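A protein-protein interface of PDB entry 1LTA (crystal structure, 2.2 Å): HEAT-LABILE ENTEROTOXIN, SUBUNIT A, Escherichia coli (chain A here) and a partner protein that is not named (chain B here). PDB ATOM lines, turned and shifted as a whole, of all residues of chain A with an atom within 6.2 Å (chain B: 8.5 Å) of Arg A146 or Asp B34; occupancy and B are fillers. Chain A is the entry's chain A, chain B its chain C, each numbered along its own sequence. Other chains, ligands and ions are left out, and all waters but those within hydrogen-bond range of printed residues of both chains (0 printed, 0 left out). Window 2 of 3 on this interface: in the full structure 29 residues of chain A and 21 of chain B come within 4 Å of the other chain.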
ATOM      1  N   SER A 122      23.793   2.450  20.111  1.00  0.00           N
ATOM      2  CA  SER A 122      24.200   2.087  18.768  1.00  0.00           C
ATOM      3  C   SER A 122      23.037   1.800  17.817  1.00  0.00           C
ATOM      4  O   SER A 122      23.221   1.655  16.603  1.00  0.00           O
ATOM      5  CB  SER A 122      25.123   0.893  18.904  1.00  0.00           C
ATOM      6  OG  SER A 122      24.645  -0.163  19.738  1.00  0.00           O
ATOM      7  N   GLN A 123      21.826   1.735  18.369  1.00  0.00           N
ATOM      8  CA  GLN A 123      20.602   1.507  17.639  1.00  0.00           C
ATOM      9  C   GLN A 123      19.946   2.837  17.287  1.00  0.00           C
ATOM     10  O   GLN A 123      18.979   2.870  16.530  1.00  0.00           O
ATOM     11  CB  GLN A 123      19.711   0.653  18.525  1.00  0.00           C
ATOM     12  CG  GLN A 123      18.418   0.194  17.840  1.00  0.00           C
ATOM     13  CD  GLN A 123      17.592  -0.786  18.630  1.00  0.00           C
ATOM     14  OE1 GLN A 123      18.009  -1.258  19.689  1.00  0.00           O
ATOM     15  NE2 GLN A 123      16.402  -1.133  18.161  1.00  0.00           N
ATOM     16  N   ARG A 141      23.128  13.076  12.745  1.00  0.00           N
ATOM     17  CA  ARG A 141      23.321  11.656  12.694  1.00  0.00           C
ATOM     18  C   ARG A 141      24.170  11.240  13.885  1.00  0.00           C
ATOM     19  O   ARG A 141      25.019  11.968  14.393  1.00  0.00           O
ATOM     20  CB  ARG A 141      23.983  11.365  11.372  1.00  0.00           C
ATOM     21  CG  ARG A 141      23.257  10.416  10.443  1.00  0.00           C
ATOM     22  CD  ARG A 141      22.977   9.052  11.120  1.00  0.00           C
ATOM     23  NE  ARG A 141      24.097   8.198  11.511  1.00  0.00           N
ATOM     24  CZ  ARG A 141      24.697   7.384  10.636  1.00  0.00           C
ATOM     25  NH1 ARG A 141      24.306   7.288   9.351  1.00  0.00           N
ATOM     26  NH2 ARG A 141      25.756   6.688  11.048  1.00  0.00           N
ATOM     27  N   GLU A 144      27.817   6.655  16.395  1.00  0.00           N
ATOM     28  CA  GLU A 144      28.000   5.277  16.819  1.00  0.00           C
ATOM     29  C   GLU A 144      26.912   4.316  16.397  1.00  0.00           C
ATOM     30  O   GLU A 144      26.888   3.166  16.874  1.00  0.00           O
ATOM     31  CB  GLU A 144      28.145   5.280  18.312  1.00  0.00           C
ATOM     32  CG  GLU A 144      29.328   6.192  18.624  1.00  0.00           C
ATOM     33  CD  GLU A 144      29.632   6.467  20.080  1.00  0.00           C
ATOM     34  OE1 GLU A 144      29.359   5.582  20.894  1.00  0.00           O
ATOM     35  OE2 GLU A 144      30.149   7.562  20.372  1.00  0.00           O
ATOM     36  N   TYR A 145      25.987   4.752  15.519  1.00  0.00           N
ATOM     37  CA  TYR A 145      24.951   3.880  14.976  1.00  0.00           C
ATOM     38  C   TYR A 145      25.632   2.726  14.190  1.00  0.00           C
ATOM     39  O   TYR A 145      26.629   2.986  13.502  1.00  0.00           O
ATOM     40  CB  TYR A 145      24.012   4.753  14.082  1.00  0.00           C
ATOM     41  CG  TYR A 145      23.025   3.937  13.230  1.00  0.00           C
ATOM     42  CD1 TYR A 145      22.035   3.215  13.862  1.00  0.00           C
ATOM     43  CD2 TYR A 145      23.141   3.894  11.859  1.00  0.00           C
ATOM     44  CE1 TYR A 145      21.170   2.466  13.127  1.00  0.00           C
ATOM     45  CE2 TYR A 145      22.267   3.132  11.107  1.00  0.00           C
ATOM     46  CZ  TYR A 145      21.296   2.438  11.770  1.00  0.00           C
ATOM     47  OH  TYR A 145      20.389   1.688  11.084  1.00  0.00           O
ATOM     48  N   ARG A 146      25.209   1.446  14.253  1.00  0.00           N
ATOM     49  CA  ARG A 146      25.886   0.373  13.528  1.00  0.00           C
ATOM     50  C   ARG A 146      25.022   0.178  12.314  1.00  0.00           C
ATOM     51  O   ARG A 146      24.027  -0.542  12.306  1.00  0.00           O
ATOM     52  CB  ARG A 146      25.936  -0.955  14.303  1.00  0.00           C
ATOM     53  CG  ARG A 146      26.330  -1.038  15.783  1.00  0.00           C
ATOM     54  CD  ARG A 146      27.747  -0.637  16.241  1.00  0.00           C
ATOM     55  NE  ARG A 146      28.823  -1.509  15.750  1.00  0.00           N
ATOM     56  CZ  ARG A 146      30.104  -1.383  16.138  1.00  0.00           C
ATOM     57  NH1 ARG A 146      30.546  -0.478  17.018  1.00  0.00           N
ATOM     58  NH2 ARG A 146      30.971  -2.149  15.510  1.00  0.00           N
ATOM     59  N   ASP A 147      25.416   0.837  11.242  1.00  0.00           N
ATOM     60  CA  ASP A 147      24.683   0.907  10.000  1.00  0.00           C
ATOM     61  C   ASP A 147      24.497  -0.464   9.371  1.00  0.00           C
ATOM     62  O   ASP A 147      23.375  -0.917   9.165  1.00  0.00           O
ATOM     63  CB  ASP A 147      25.477   1.892   9.132  1.00  0.00           C
ATOM     64  CG  ASP A 147      24.702   2.568   7.994  1.00  0.00           C
ATOM     65  OD1 ASP A 147      24.532   1.936   6.950  1.00  0.00           O
ATOM     66  OD2 ASP A 147      24.292   3.734   8.149  1.00  0.00           O
ATOM     67  N   ARG A 148      25.597  -1.197   9.200  1.00  0.00           N
ATOM     68  CA  ARG A 148      25.542  -2.491   8.587  1.00  0.00           C
ATOM     69  C   ARG A 148      24.703  -3.467   9.397  1.00  0.00           C
ATOM     70  O   ARG A 148      23.860  -4.191   8.830  1.00  0.00           O
ATOM     71  CB  ARG A 148      26.958  -3.021   8.436  1.00  0.00           C
ATOM     72  CG  ARG A 148      26.996  -4.330   7.667  1.00  0.00           C
ATOM     73  CD  ARG A 148      28.359  -5.011   7.654  1.00  0.00           C
ATOM     74  NE  ARG A 148      29.362  -4.210   6.966  1.00  0.00           N
ATOM     75  CZ  ARG A 148      30.442  -3.714   7.589  1.00  0.00           C
ATOM     76  NH1 ARG A 148      30.665  -3.929   8.891  1.00  0.00           N
ATOM     77  NH2 ARG A 148      31.313  -2.994   6.884  1.00  0.00           N
ATOM     78  N   TYR A 149      24.931  -3.494  10.707  1.00  0.00           N
ATOM     79  CA  TYR A 149      24.184  -4.417  11.560  1.00  0.00           C
ATOM     80  C   TYR A 149      22.691  -4.149  11.564  1.00  0.00           C
ATOM     81  O   TYR A 149      21.884  -5.049  11.306  1.00  0.00           O
ATOM     82  CB  TYR A 149      24.688  -4.341  13.003  1.00  0.00           C
ATOM     83  CG  TYR A 149      24.011  -5.382  13.887  1.00  0.00           C
ATOM     84  CD1 TYR A 149      24.188  -6.711  13.577  1.00  0.00           C
ATOM     85  CD2 TYR A 149      23.199  -5.056  14.960  1.00  0.00           C
ATOM     86  CE1 TYR A 149      23.564  -7.699  14.315  1.00  0.00           C
ATOM     87  CE2 TYR A 149      22.586  -6.047  15.702  1.00  0.00           C
ATOM     88  CZ  TYR A 149      22.776  -7.357  15.362  1.00  0.00           C
ATOM     89  OH  TYR A 149      22.175  -8.365  16.060  1.00  0.00           O
ATOM     90  N   TYR A 150      22.299  -2.901  11.878  1.00  0.00           N
ATOM     91  CA  TYR A 150      20.878  -2.556  11.916  1.00  0.00           C
ATOM     92  C   TYR A 150      20.153  -2.429  10.582  1.00  0.00           C
ATOM     93  O   TYR A 150      18.940  -2.575  10.521  1.00  0.00           O
ATOM     94  CB  TYR A 150      20.752  -1.286  12.696  1.00  0.00           C
ATOM     95  CG  TYR A 150      20.915  -1.646  14.164  1.00  0.00           C
ATOM     96  CD1 TYR A 150      20.012  -2.513  14.777  1.00  0.00           C
ATOM     97  CD2 TYR A 150      21.980  -1.142  14.877  1.00  0.00           C
ATOM     98  CE1 TYR A 150      20.171  -2.878  16.106  1.00  0.00           C
ATOM     99  CE2 TYR A 150      22.133  -1.506  16.199  1.00  0.00           C
ATOM    100  CZ  TYR A 150      21.237  -2.361  16.795  1.00  0.00           C
ATOM    101  OH  TYR A 150      21.428  -2.714  18.108  1.00  0.00           O
ATOM    102  N   ARG A 151      20.887  -2.238   9.495  1.00  0.00           N
ATOM    103  CA  ARG A 151      20.378  -2.108   8.147  1.00  0.00           C
ATOM    104  C   ARG A 151      19.133  -2.915   7.825  1.00  0.00           C
ATOM    105  O   ARG A 151      18.055  -2.427   7.523  1.00  0.00           O
ATOM    106  CB  ARG A 151      21.515  -2.499   7.168  1.00  0.00           C
ATOM    107  CG  ARG A 151      21.421  -1.888   5.757  1.00  0.00           C
ATOM    108  CD  ARG A 151      22.660  -2.107   4.842  1.00  0.00           C
ATOM    109  NE  ARG A 151      23.875  -1.361   5.221  1.00  0.00           N
ATOM    110  CZ  ARG A 151      25.119  -1.869   5.065  1.00  0.00           C
ATOM    111  NH1 ARG A 151      25.273  -3.101   4.547  1.00  0.00           N
ATOM    112  NH2 ARG A 151      26.203  -1.158   5.472  1.00  0.00           N
ATOM    113  N   LYS B  26      23.779  -9.858  21.582  1.00  0.00           N
ATOM    114  CA  LYS B  26      23.936  -9.450  20.179  1.00  0.00           C
ATOM    115  C   LYS B  26      24.579  -8.071  20.079  1.00  0.00           C
ATOM    116  O   LYS B  26      25.384  -7.819  19.174  1.00  0.00           O
ATOM    117  CB  LYS B  26      22.603  -9.363  19.460  1.00  0.00           C
ATOM    118  CG  LYS B  26      21.772 -10.603  19.402  1.00  0.00           C
ATOM    119  CD  LYS B  26      22.549 -11.528  18.513  1.00  0.00           C
ATOM    120  CE  LYS B  26      21.804 -12.833  18.301  1.00  0.00           C
ATOM    121  NZ  LYS B  26      21.724 -13.171  16.884  1.00  0.00           N
ATOM    122  N   VAL B  27      24.221  -7.152  21.002  1.00  0.00           N
ATOM    123  CA  VAL B  27      24.797  -5.806  21.060  1.00  0.00           C
ATOM    124  C   VAL B  27      26.273  -5.885  21.498  1.00  0.00           C
ATOM    125  O   VAL B  27      27.142  -5.241  20.891  1.00  0.00           O
ATOM    126  CB  VAL B  27      23.961  -4.909  22.046  1.00  0.00           C
ATOM    127  CG1 VAL B  27      24.549  -3.508  22.092  1.00  0.00           C
ATOM    128  CG2 VAL B  27      22.513  -4.760  21.579  1.00  0.00           C
ATOM    129  N   LYS B  28      26.597  -6.658  22.545  1.00  0.00           N
ATOM    130  CA  LYS B  28      27.961  -6.861  22.980  1.00  0.00           C
ATOM    131  C   LYS B  28      28.761  -7.500  21.859  1.00  0.00           C
ATOM    132  O   LYS B  28      29.909  -7.094  21.682  1.00  0.00           O
ATOM    133  CB  LYS B  28      28.010  -7.753  24.233  1.00  0.00           C
ATOM    134  CG  LYS B  28      27.451  -7.047  25.466  1.00  0.00           C
ATOM    135  CD  LYS B  28      27.729  -7.862  26.697  1.00  0.00           C
ATOM    136  CE  LYS B  28      27.282  -7.164  27.960  1.00  0.00           C
ATOM    137  NZ  LYS B  28      27.574  -7.932  29.166  1.00  0.00           N
ATOM    138  N   ARG B  29      28.253  -8.424  21.044  1.00  0.00           N
ATOM    139  CA  ARG B  29      29.027  -8.978  19.947  1.00  0.00           C
ATOM    140  C   ARG B  29      29.336  -7.906  18.945  1.00  0.00           C
ATOM    141  O   ARG B  29      30.312  -8.025  18.217  1.00  0.00           O
ATOM    142  CB  ARG B  29      28.284 -10.054  19.216  1.00  0.00           C
ATOM    143  CG  ARG B  29      28.259 -11.320  19.996  1.00  0.00           C
ATOM    144  CD  ARG B  29      27.153 -12.215  19.495  1.00  0.00           C
ATOM    145  NE  ARG B  29      27.438 -12.780  18.184  1.00  0.00           N
ATOM    146  CZ  ARG B  29      26.767 -13.838  17.686  1.00  0.00           C
ATOM    147  NH1 ARG B  29      25.803 -14.431  18.378  1.00  0.00           N
ATOM    148  NH2 ARG B  29      27.027 -14.322  16.460  1.00  0.00           N
ATOM    149  N   GLN B  30      28.506  -6.870  18.864  1.00  0.00           N
ATOM    150  CA  GLN B  30      28.791  -5.747  17.977  1.00  0.00           C
ATOM    151  C   GLN B  30      29.773  -4.802  18.611  1.00  0.00           C
ATOM    152  O   GLN B  30      30.840  -4.613  18.026  1.00  0.00           O
ATOM    153  CB  GLN B  30      27.573  -4.882  17.624  1.00  0.00           C
ATOM    154  CG  GLN B  30      26.610  -5.624  16.726  1.00  0.00           C
ATOM    155  CD  GLN B  30      27.206  -5.956  15.358  1.00  0.00           C
ATOM    156  OE1 GLN B  30      27.681  -5.103  14.608  1.00  0.00           O
ATOM    157  NE2 GLN B  30      27.163  -7.223  14.985  1.00  0.00           N
ATOM    158  N   ILE B  31      29.506  -4.222  19.786  1.00  0.00           N
ATOM    159  CA  ILE B  31      30.434  -3.234  20.264  1.00  0.00           C
ATOM    160  C   ILE B  31      31.679  -3.834  20.881  1.00  0.00           C
ATOM    161  O   ILE B  31      32.747  -3.242  20.693  1.00  0.00           O
ATOM    162  CB  ILE B  31      29.725  -2.280  21.243  1.00  0.00           C
ATOM    163  CG1 ILE B  31      29.005  -2.973  22.330  1.00  0.00           C
ATOM    164  CG2 ILE B  31      28.672  -1.512  20.437  1.00  0.00           C
ATOM    165  CD1 ILE B  31      28.340  -1.941  23.246  1.00  0.00           C
ATOM    166  N   PHE B  32      31.699  -5.005  21.499  1.00  0.00           N
ATOM    167  CA  PHE B  32      32.968  -5.480  22.035  1.00  0.00           C
ATOM    168  C   PHE B  32      33.955  -5.986  21.013  1.00  0.00           C
ATOM    169  O   PHE B  32      35.168  -5.921  21.237  1.00  0.00           O
ATOM    170  CB  PHE B  32      32.725  -6.560  23.062  1.00  0.00           C
ATOM    171  CG  PHE B  32      32.088  -6.007  24.319  1.00  0.00           C
ATOM    172  CD1 PHE B  32      31.850  -4.659  24.475  1.00  0.00           C
ATOM    173  CD2 PHE B  32      31.740  -6.881  25.324  1.00  0.00           C
ATOM    174  CE1 PHE B  32      31.258  -4.194  25.635  1.00  0.00           C
ATOM    175  CE2 PHE B  32      31.149  -6.419  26.481  1.00  0.00           C
ATOM    176  CZ  PHE B  32      30.905  -5.070  26.642  1.00  0.00           C
ATOM    177  N   SER B  33      33.479  -6.423  19.865  1.00  0.00           N
ATOM    178  CA  SER B  33      34.358  -6.900  18.846  1.00  0.00           C
ATOM    179  C   SER B  33      35.256  -5.828  18.259  1.00  0.00           C
ATOM    180  O   SER B  33      36.271  -6.179  17.646  1.00  0.00           O
ATOM    181  CB  SER B  33      33.505  -7.533  17.786  1.00  0.00           C
ATOM    182  OG  SER B  33      32.936  -8.694  18.382  1.00  0.00           O
ATOM    183  N   ASP B  34      34.980  -4.523  18.375  1.00  0.00           N
ATOM    184  CA  ASP B  34      35.909  -3.513  17.867  1.00  0.00           C
ATOM    185  C   ASP B  34      37.197  -3.502  18.677  1.00  0.00           C
ATOM    186  O   ASP B  34      38.216  -3.040  18.172  1.00  0.00           O
ATOM    187  CB  ASP B  34      35.353  -2.091  17.921  1.00  0.00           C
ATOM    188  CG  ASP B  34      34.057  -1.856  17.144  1.00  0.00           C
ATOM    189  OD1 ASP B  34      33.705  -2.575  16.202  1.00  0.00           O
ATOM    190  OD2 ASP B  34      33.342  -0.930  17.494  1.00  0.00           O
ATOM    191  N   TYR B  35      37.210  -4.034  19.900  1.00  0.00           N
ATOM    192  CA  TYR B  35      38.412  -4.081  20.728  1.00  0.00           C
ATOM    193  C   TYR B  35      39.269  -5.337  20.565  1.00  0.00           C
ATOM    194  O   TYR B  35      40.315  -5.445  21.210  1.00  0.00           O
ATOM    195  CB  TYR B  35      38.045  -4.010  22.174  1.00  0.00           C
ATOM    196  CG  TYR B  35      37.180  -2.807  22.461  1.00  0.00           C
ATOM    197  CD1 TYR B  35      37.728  -1.540  22.394  1.00  0.00           C
ATOM    198  CD2 TYR B  35      35.878  -3.026  22.855  1.00  0.00           C
ATOM    199  CE1 TYR B  35      36.963  -0.460  22.735  1.00  0.00           C
ATOM    200  CE2 TYR B  35      35.112  -1.951  23.203  1.00  0.00           C
ATOM    201  CZ  TYR B  35      35.663  -0.683  23.137  1.00  0.00           C
ATOM    202  OH  TYR B  35      34.882   0.388  23.534  1.00  0.00           O
ATOM    203  N   GLN B  36      38.804  -6.339  19.803  1.00  0.00           N
ATOM    204  CA  GLN B  36      39.497  -7.607  19.605  1.00  0.00           C
ATOM    205  C   GLN B  36      40.766  -7.380  18.777  1.00  0.00           C
ATOM    206  O   GLN B  36      40.682  -6.899  17.651  1.00  0.00           O
ATOM    207  CB  GLN B  36      38.512  -8.583  18.910  1.00  0.00           C
ATOM    208  CG  GLN B  36      39.010  -9.958  18.481  1.00  0.00           C
ATOM    209  CD  GLN B  36      39.841 -10.751  19.483  1.00  0.00           C
ATOM    210  OE1 GLN B  36      40.722 -11.518  19.080  1.00  0.00           O
ATOM    211  NE2 GLN B  36      39.632 -10.630  20.776  1.00  0.00           N
ATOM    212  N   SER B  37      41.933  -7.754  19.297  1.00  0.00           N
ATOM    213  CA  SER B  37      43.185  -7.530  18.616  1.00  0.00           C
ATOM    214  C   SER B  37      43.711  -8.929  18.337  1.00  0.00           C
ATOM    215  O   SER B  37      43.629  -9.854  19.163  1.00  0.00           O
ATOM    216  CB  SER B  37      44.124  -6.769  19.526  1.00  0.00           C
ATOM    217  OG  SER B  37      45.090  -6.022  18.794  1.00  0.00           O
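NH2 of Arg A146 is in salt-bridge range of OD1 of Asp B34.
Asp B34 touches just one residue of chain A: Arg A146 (2.9 Å).
Of the printed residues of chain B, Tyr A149 touches Lys B26 (3.6 Å) and Gln B30 (3.3 Å).
Of the printed residues of chain A, Lys B26 touches Tyr A149 (3.6 Å).
Printed residues of chain A within 4 Å of Gln B30: Arg A146 (3.5 Å) and Tyr A149 (3.3 Å).
Arg B29 touches none of the printed residues of chain A.
Gln B36 touches none of the printed residues of chain A.
The nearest residue of chain B that does not touch Arg A146 is Ile B31 (4.03 Å).
The nearest printed residue of chain A that does not touch Asp B34 is Glu A144 (7.7 Å).
Printed residues of chain A that touch a printed residue of chain B: Arg A146 and Tyr A149.
Hydrophobic or aromatic side chains of chain A within 4 Å of the printed part of chain B: Tyr A149.
Of the 12 printed residues of chain B, 3 touch a printed residue of chain A.
Printed residues of chain B that touch a printed residue of chain A: Lys B26, Gln B30 and Asp B34.
Among the printed residues, Asp or Glu carboxylates within 4 Å of a Lys or Arg side-chain nitrogen of the other chain: Arg A146 with Asp B34 (2.9 Å).
Among the printed residues, pairs that only touch across the chains: Tyr A149 with Gln B30 (3.3 Å), Arg A146 with Gln B30 (3.5 Å) and Tyr A149 with Lys B26 (3.6 Å).
The backbone carbonyl oxygen (O) of Ser A122 is in hydrogen-bond range of the backbone NH (N) of Arg A146 (3.1 Å).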
